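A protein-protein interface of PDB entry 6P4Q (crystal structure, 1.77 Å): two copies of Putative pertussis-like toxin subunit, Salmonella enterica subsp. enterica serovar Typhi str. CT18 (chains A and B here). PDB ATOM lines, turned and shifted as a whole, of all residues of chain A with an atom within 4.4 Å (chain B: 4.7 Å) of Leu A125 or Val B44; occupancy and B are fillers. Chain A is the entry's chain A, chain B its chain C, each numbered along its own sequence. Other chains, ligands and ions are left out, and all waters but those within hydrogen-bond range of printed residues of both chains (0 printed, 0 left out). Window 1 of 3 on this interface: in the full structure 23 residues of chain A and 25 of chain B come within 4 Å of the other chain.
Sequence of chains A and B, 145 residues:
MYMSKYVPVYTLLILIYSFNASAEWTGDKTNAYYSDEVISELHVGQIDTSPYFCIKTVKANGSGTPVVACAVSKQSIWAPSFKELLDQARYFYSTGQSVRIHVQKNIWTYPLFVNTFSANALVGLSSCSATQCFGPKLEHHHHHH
Ile A101 touches none of the printed residues of chain B.
Printed residues of chain B within 4 Å of Gly A124: Val B44 (3.3 Å).
Of the printed residues of chain B, Ser A127 touches Leu B42.
Printed residues of chain A within 4 Å of Leu B42: Gln A88 (3.4 Å), Ser A126 (3.9 Å) and Ser A127 (2.9 Å).
Of the printed residues of chain A, His B43 touches Leu A125 (3.4 Å) and Ser A126 (2.8 Å).
Printed residues of chain A within 4 Å of Val B44: Glu A84, Gln A88, Gly A124 and Leu A125.
Printed residues of chain A within 4 Å of Gly B45: Glu A84 (3.5 Å).
The nearest residue of chain B that does not touch Leu A125 is Leu B42 (4.3 Å).
NE2 of His B43 is in hydrogen-bond range of OH of Tyr B52 (2.7 Å).
N of Arg A100 sits at hydrogen-bond distance from O of Ser A126 (2.8 Å).
A ring nitrogen (NE2) of His A102 is in hydrogen-bond range of the side-chain hydroxyl (OG) of Ser A126 (2.8 Å).
O of Gly B45 is in hydrogen-bond range of N of Tyr B52 (3.0 Å).
O of Gly A124 lies within hydrogen-bond range of N of His A102 (3.0 Å).
Glu A84 touches Val B44 (OE2 to CB, 3.2 Å).
Gly B45 touches Glu A84 (O to OE2, 3.5 Å).
Gln A88 touches Leu B42.
OE1 of Gln A88 touches CG1 of Val B44 (3.7 Å).
Gly A124 touches Val B44 (CA to O, 3.3 Å).
Leu A125 touches His B43.
Ser A126 touches Leu B42 (C to O, 3.9 Å).
No position is printed for both chains.
The side-chain carboxylate (OE2) of Glu A84 lies close to the backbone carbonyl oxygen (O) of Tyr B52 (2.5 Å).
N of Val B44 is in hydrogen-bond range of O of Leu A125 (2.9 Å).
The side-chain amide oxygen of Gln A88 is in hydrogen-bond range of the guanidinium group of Arg B90, at 2.8 Å.
O of Glu A84 sits at hydrogen-bond distance from NH2 of Arg B90 (3.3 Å).
ND1 of His B43 is in hydrogen-bond range of OG of Ser A126.
The side-chain hydroxyl (OG) of Ser A127 is in hydrogen-bond range of the backbone NH (N) of Leu B42.
Of the 7 printed residues of chain B, 6 touch a printed residue of chain A.
Printed residues of chain B that touch a printed residue of chain A: Leu B42, His B43, Val B44, Gly B45, Tyr B52 and Arg B90.
Hydrophobic or aromatic side chains of chain B within 4 Å of the printed part of chain A: Leu B42, His B43 and Val B44.
Printed residues of chain A that touch a printed residue of chain B: Glu A84, Gln A88, Gly A124, Leu A125, Ser A126 and Ser A127.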
ATOM      1  N   ILE A  55     -21.996 -18.069 -29.676  1.00  0.00           N
ATOM      2  CA  ILE A  55     -21.611 -18.387 -28.313  1.00  0.00           C
ATOM      3  C   ILE A  55     -20.111 -18.622 -28.277  1.00  0.00           C
ATOM      4  O   ILE A  55     -19.487 -19.013 -29.274  1.00  0.00           O
ATOM      5  CB  ILE A  55     -22.363 -19.617 -27.764  1.00  0.00           C
ATOM      6  CG1 ILE A  55     -22.247 -20.802 -28.731  1.00  0.00           C
ATOM      7  CG2 ILE A  55     -23.825 -19.283 -27.575  1.00  0.00           C
ATOM      8  CD1 ILE A  55     -22.828 -22.116 -28.161  1.00  0.00           C
ATOM      9  N   GLU A  84     -34.236 -23.729 -31.910  1.00  0.00           N
ATOM     10  CA  GLU A  84     -33.926 -24.769 -30.938  1.00  0.00           C
ATOM     11  C   GLU A  84     -32.542 -24.554 -30.337  1.00  0.00           C
ATOM     12  O   GLU A  84     -32.351 -24.661 -29.120  1.00  0.00           O
ATOM     13  CB  GLU A  84     -34.012 -26.134 -31.624  1.00  0.00           C
ATOM     14  CG  GLU A  84     -33.658 -27.295 -30.731  1.00  0.00           C
ATOM     15  CD  GLU A  84     -33.966 -28.630 -31.382  1.00  0.00           C
ATOM     16  OE1 GLU A  84     -34.965 -28.734 -32.121  1.00  0.00           O
ATOM     17  OE2 GLU A  84     -33.211 -29.578 -31.153  1.00  0.00           O
ATOM     18  N   LEU A  85     -31.552 -24.272 -31.191  1.00  0.00           N
ATOM     19  CA  LEU A  85     -30.189 -24.070 -30.710  1.00  0.00           C
ATOM     20  C   LEU A  85     -30.067 -22.787 -29.893  1.00  0.00           C
ATOM     21  O   LEU A  85     -29.325 -22.742 -28.907  1.00  0.00           O
ATOM     22  CB  LEU A  85     -29.221 -24.033 -31.895  1.00  0.00           C
ATOM     23  CG  LEU A  85     -29.019 -25.351 -32.645  1.00  0.00           C
ATOM     24  CD1 LEU A  85     -28.385 -25.085 -34.009  1.00  0.00           C
ATOM     25  CD2 LEU A  85     -28.141 -26.287 -31.832  1.00  0.00           C
ATOM     26  N   GLN A  88     -31.635 -23.508 -26.511  1.00  0.00           N
ATOM     27  CA  GLN A  88     -30.811 -24.382 -25.680  1.00  0.00           C
ATOM     28  C   GLN A  88     -29.527 -23.694 -25.259  1.00  0.00           C
ATOM     29  O   GLN A  88     -29.069 -23.865 -24.121  1.00  0.00           O
ATOM     30  CB  GLN A  88     -30.474 -25.680 -26.394  1.00  0.00           C
ATOM     31  CG  GLN A  88     -30.117 -26.779 -25.410  1.00  0.00           C
ATOM     32  CD  GLN A  88     -31.272 -27.064 -24.488  1.00  0.00           C
ATOM     33  OE1 GLN A  88     -32.412 -27.229 -24.942  1.00  0.00           O
ATOM     34  NE2 GLN A  88     -31.010 -27.059 -23.179  1.00  0.00           N
ATOM     35  N   ALA A  89     -28.924 -22.927 -26.166  1.00  0.00           N
ATOM     36  CA  ALA A  89     -27.732 -22.172 -25.803  1.00  0.00           C
ATOM     37  C   ALA A  89     -28.030 -21.231 -24.646  1.00  0.00           C
ATOM     38  O   ALA A  89     -27.232 -21.114 -23.710  1.00  0.00           O
ATOM     39  CB  ALA A  89     -27.214 -21.398 -27.016  1.00  0.00           C
ATOM     40  N   PHE A  92     -28.251 -23.345 -21.286  1.00  0.00           N
ATOM     41  CA  PHE A  92     -26.931 -23.761 -20.810  1.00  0.00           C
ATOM     42  C   PHE A  92     -26.066 -22.562 -20.411  1.00  0.00           C
ATOM     43  O   PHE A  92     -25.262 -22.660 -19.481  1.00  0.00           O
ATOM     44  CB  PHE A  92     -26.237 -24.602 -21.887  1.00  0.00           C
ATOM     45  CG  PHE A  92     -26.843 -25.987 -22.086  1.00  0.00           C
ATOM     46  CD1 PHE A  92     -27.578 -26.596 -21.083  1.00  0.00           C
ATOM     47  CD2 PHE A  92     -26.667 -26.670 -23.288  1.00  0.00           C
ATOM     48  CE1 PHE A  92     -28.113 -27.880 -21.260  1.00  0.00           C
ATOM     49  CE2 PHE A  92     -27.201 -27.948 -23.479  1.00  0.00           C
ATOM     50  CZ  PHE A  92     -27.929 -28.551 -22.461  1.00  0.00           C
ATOM     51  N   ARG A 100     -21.171 -30.457 -24.126  1.00  0.00           N
ATOM     52  CA  ARG A 100     -20.393 -30.693 -25.337  1.00  0.00           C
ATOM     53  C   ARG A 100     -20.966 -29.801 -26.432  1.00  0.00           C
ATOM     54  O   ARG A 100     -22.179 -29.801 -26.653  1.00  0.00           O
ATOM     55  CB  ARG A 100     -20.445 -32.165 -25.762  1.00  0.00           C
ATOM     56  CG  ARG A 100     -19.734 -32.445 -27.091  1.00  0.00           C
ATOM     57  CD  ARG A 100     -19.822 -33.926 -27.453  1.00  0.00           C
ATOM     58  NE  ARG A 100     -19.049 -34.739 -26.509  1.00  0.00           N
ATOM     59  CZ  ARG A 100     -19.308 -36.010 -26.236  1.00  0.00           C
ATOM     60  NH1 ARG A 100     -20.312 -36.625 -26.849  1.00  0.00           N
ATOM     61  NH2 ARG A 100     -18.564 -36.661 -25.338  1.00  0.00           N
ATOM     62  N   ILE A 101     -20.107 -29.037 -27.102  1.00  0.00           N
ATOM     63  CA  ILE A 101     -20.524 -28.204 -28.228  1.00  0.00           C
ATOM     64  C   ILE A 101     -20.127 -28.904 -29.520  1.00  0.00           C
ATOM     65  O   ILE A 101     -19.018 -29.442 -29.631  1.00  0.00           O
ATOM     66  CB  ILE A 101     -19.928 -26.784 -28.137  1.00  0.00           C
ATOM     67  CG1 ILE A 101     -20.315 -25.959 -29.366  1.00  0.00           C
ATOM     68  CG2 ILE A 101     -18.425 -26.823 -27.887  1.00  0.00           C
ATOM     69  CD1 ILE A 101     -20.028 -24.440 -29.222  1.00  0.00           C
ATOM     70  N   HIS A 102     -21.045 -28.935 -30.484  1.00  0.00           N
ATOM     71  CA  HIS A 102     -20.815 -29.560 -31.786  1.00  0.00           C
ATOM     72  C   HIS A 102     -20.848 -28.486 -32.861  1.00  0.00           C
ATOM     73  O   HIS A 102     -21.806 -27.713 -32.928  1.00  0.00           O
ATOM     74  CB  HIS A 102     -21.885 -30.610 -32.094  1.00  0.00           C
ATOM     75  CG  HIS A 102     -22.095 -31.617 -31.002  1.00  0.00           C
ATOM     76  ND1 HIS A 102     -21.642 -32.913 -31.097  1.00  0.00           N
ATOM     77  CD2 HIS A 102     -22.740 -31.528 -29.812  1.00  0.00           C
ATOM     78  CE1 HIS A 102     -21.987 -33.579 -30.006  1.00  0.00           C
ATOM     79  NE2 HIS A 102     -22.662 -32.764 -29.214  1.00  0.00           N
ATOM     80  N   LEU A 122     -22.748 -23.589 -35.424  1.00  0.00           N
ATOM     81  CA  LEU A 122     -23.186 -24.388 -34.287  1.00  0.00           C
ATOM     82  C   LEU A 122     -24.198 -25.412 -34.777  1.00  0.00           C
ATOM     83  O   LEU A 122     -25.209 -25.040 -35.392  1.00  0.00           O
ATOM     84  CB  LEU A 122     -23.807 -23.481 -33.225  1.00  0.00           C
ATOM     85  CG  LEU A 122     -24.387 -24.202 -32.007  1.00  0.00           C
ATOM     86  CD1 LEU A 122     -23.272 -24.849 -31.215  1.00  0.00           C
ATOM     87  CD2 LEU A 122     -25.141 -23.200 -31.139  1.00  0.00           C
ATOM     88  N   GLY A 124     -24.972 -28.430 -32.681  1.00  0.00           N
ATOM     89  CA  GLY A 124     -25.581 -29.198 -31.602  1.00  0.00           C
ATOM     90  C   GLY A 124     -25.016 -28.816 -30.251  1.00  0.00           C
ATOM     91  O   GLY A 124     -23.935 -28.231 -30.143  1.00  0.00           O
ATOM     92  N   LEU A 125     -25.790 -29.150 -29.215  1.00  0.00           N
ATOM     93  CA  LEU A 125     -25.386 -28.942 -27.829  1.00  0.00           C
ATOM     94  C   LEU A 125     -25.844 -30.132 -27.002  1.00  0.00           C
ATOM     95  O   LEU A 125     -27.014 -30.516 -27.075  1.00  0.00           O
ATOM     96  CB  LEU A 125     -25.997 -27.662 -27.260  1.00  0.00           C
ATOM     97  CG  LEU A 125     -25.442 -26.353 -27.818  1.00  0.00           C
ATOM     98  CD1 LEU A 125     -26.360 -25.204 -27.433  1.00  0.00           C
ATOM     99  CD2 LEU A 125     -24.035 -26.136 -27.265  1.00  0.00           C
ATOM    100  N   SER A 126     -24.941 -30.678 -26.186  1.00  0.00           N
ATOM    101  CA  SER A 126     -25.216 -31.849 -25.362  1.00  0.00           C
ATOM    102  C   SER A 126     -24.915 -31.521 -23.905  1.00  0.00           C
ATOM    103  O   SER A 126     -23.855 -30.971 -23.602  1.00  0.00           O
ATOM    104  CB  SER A 126     -24.359 -33.046 -25.789  1.00  0.00           C
ATOM    105  OG  SER A 126     -24.467 -33.323 -27.175  1.00  0.00           O
ATOM    106  N   SER A 127     -25.823 -31.886 -23.010  1.00  0.00           N
ATOM    107  CA  SER A 127     -25.470 -31.811 -21.597  1.00  0.00           C
ATOM    108  C   SER A 127     -24.391 -32.847 -21.280  1.00  0.00           C
ATOM    109  O   SER A 127     -24.207 -33.842 -21.994  1.00  0.00           O
ATOM    110  CB  SER A 127     -26.708 -32.010 -20.715  1.00  0.00           C
ATOM    111  OG  SER A 127     -27.247 -33.307 -20.888  1.00  0.00           O
ATOM    112  N   LEU B  42     -30.005 -33.790 -21.588  1.00  0.00           N
ATOM    113  CA  LEU B  42     -30.757 -33.225 -22.700  1.00  0.00           C
ATOM    114  C   LEU B  42     -29.778 -32.880 -23.817  1.00  0.00           C
ATOM    115  O   LEU B  42     -28.701 -32.341 -23.559  1.00  0.00           O
ATOM    116  CB  LEU B  42     -31.526 -31.979 -22.237  1.00  0.00           C
ATOM    117  CG  LEU B  42     -32.249 -31.107 -23.257  1.00  0.00           C
ATOM    118  CD1 LEU B  42     -33.366 -31.885 -23.890  1.00  0.00           C
ATOM    119  CD2 LEU B  42     -32.789 -29.862 -22.546  1.00  0.00           C
ATOM    120  N   HIS B  43     -30.148 -33.191 -25.057  1.00  0.00           N
ATOM    121  CA  HIS B  43     -29.305 -32.927 -26.217  1.00  0.00           C
ATOM    122  C   HIS B  43     -30.170 -32.344 -27.322  1.00  0.00           C
ATOM    123  O   HIS B  43     -31.297 -32.800 -27.517  1.00  0.00           O
ATOM    124  CB  HIS B  43     -28.621 -34.222 -26.713  1.00  0.00           C
ATOM    125  CG  HIS B  43     -28.153 -34.162 -28.138  1.00  0.00           C
ATOM    126  ND1 HIS B  43     -26.850 -33.876 -28.488  1.00  0.00           N
ATOM    127  CD2 HIS B  43     -28.811 -34.383 -29.303  1.00  0.00           C
ATOM    128  CE1 HIS B  43     -26.731 -33.899 -29.804  1.00  0.00           C
ATOM    129  NE2 HIS B  43     -27.904 -34.219 -30.322  1.00  0.00           N
ATOM    130  N   VAL B  44     -29.660 -31.341 -28.046  1.00  0.00           N
ATOM    131  CA  VAL B  44     -30.359 -30.828 -29.221  1.00  0.00           C
ATOM    132  C   VAL B  44     -29.440 -30.903 -30.432  1.00  0.00           C
ATOM    133  O   VAL B  44     -28.236 -30.632 -30.336  1.00  0.00           O
ATOM    134  CB  VAL B  44     -30.860 -29.382 -29.034  1.00  0.00           C
ATOM    135  CG1 VAL B  44     -31.905 -29.321 -27.916  1.00  0.00           C
ATOM    136  CG2 VAL B  44     -29.705 -28.467 -28.732  1.00  0.00           C
ATOM    137  N   GLY B  45     -30.024 -31.239 -31.578  1.00  0.00           N
ATOM    138  CA  GLY B  45     -29.284 -31.301 -32.818  1.00  0.00           C
ATOM    139  C   GLY B  45     -30.214 -31.235 -34.009  1.00  0.00           C
ATOM    140  O   GLY B  45     -31.358 -30.783 -33.899  1.00  0.00           O
ATOM    141  N   TYR B  52     -34.027 -32.043 -33.893  1.00  0.00           N
ATOM    142  CA  TYR B  52     -34.444 -33.120 -32.999  1.00  0.00           C
ATOM    143  C   TYR B  52     -33.903 -32.844 -31.603  1.00  0.00           C
ATOM    144  O   TYR B  52     -32.964 -32.073 -31.424  1.00  0.00           O
ATOM    145  CB  TYR B  52     -33.970 -34.500 -33.499  1.00  0.00           C
ATOM    146  CG  TYR B  52     -32.488 -34.751 -33.293  1.00  0.00           C
ATOM    147  CD1 TYR B  52     -31.568 -34.394 -34.269  1.00  0.00           C
ATOM    148  CD2 TYR B  52     -32.007 -35.334 -32.109  1.00  0.00           C
ATOM    149  CE1 TYR B  52     -30.207 -34.598 -34.086  1.00  0.00           C
ATOM    150  CE2 TYR B  52     -30.658 -35.530 -31.914  1.00  0.00           C
ATOM    151  CZ  TYR B  52     -29.757 -35.167 -32.914  1.00  0.00           C
ATOM    152  OH  TYR B  52     -28.395 -35.355 -32.728  1.00  0.00           O
ATOM    153  N   PHE B  53     -34.486 -33.504 -30.609  1.00  0.00           N
ATOM    154  CA  PHE B  53     -33.869 -33.513 -29.286  1.00  0.00           C
ATOM    155  C   PHE B  53     -33.977 -34.910 -28.699  1.00  0.00           C
ATOM    156  O   PHE B  53     -34.802 -35.719 -29.117  1.00  0.00           O
ATOM    157  CB  PHE B  53     -34.491 -32.474 -28.337  1.00  0.00           C
ATOM    158  CG  PHE B  53     -35.819 -32.874 -27.773  1.00  0.00           C
ATOM    159  CD1 PHE B  53     -36.989 -32.644 -28.486  1.00  0.00           C
ATOM    160  CD2 PHE B  53     -35.906 -33.460 -26.521  1.00  0.00           C
ATOM    161  CE1 PHE B  53     -38.218 -33.004 -27.974  1.00  0.00           C
ATOM    162  CE2 PHE B  53     -37.152 -33.816 -25.996  1.00  0.00           C
ATOM    163  CZ  PHE B  53     -38.301 -33.578 -26.726  1.00  0.00           C
ATOM    164  N   ARG B  90     -37.870 -29.794 -21.241  1.00  0.00           N
ATOM    165  CA  ARG B  90     -37.025 -28.763 -20.651  1.00  0.00           C
ATOM    166  C   ARG B  90     -37.516 -28.397 -19.262  1.00  0.00           C
ATOM    167  O   ARG B  90     -36.719 -28.244 -18.332  1.00  0.00           O
ATOM    168  CB  ARG B  90     -36.999 -27.530 -21.548  1.00  0.00           C
ATOM    169  CG  ARG B  90     -36.107 -27.695 -22.777  1.00  0.00           C
ATOM    170  CD  ARG B  90     -36.139 -26.457 -23.672  1.00  0.00           C
ATOM    171  NE  ARG B  90     -35.085 -26.512 -24.685  1.00  0.00           N
ATOM    172  CZ  ARG B  90     -35.189 -25.978 -25.901  1.00  0.00           C
ATOM    173  NH1 ARG B  90     -36.307 -25.347 -26.254  1.00  0.00           N
ATOM    174  NH2 ARG B  90     -34.183 -26.080 -26.761  1.00  0.00           N
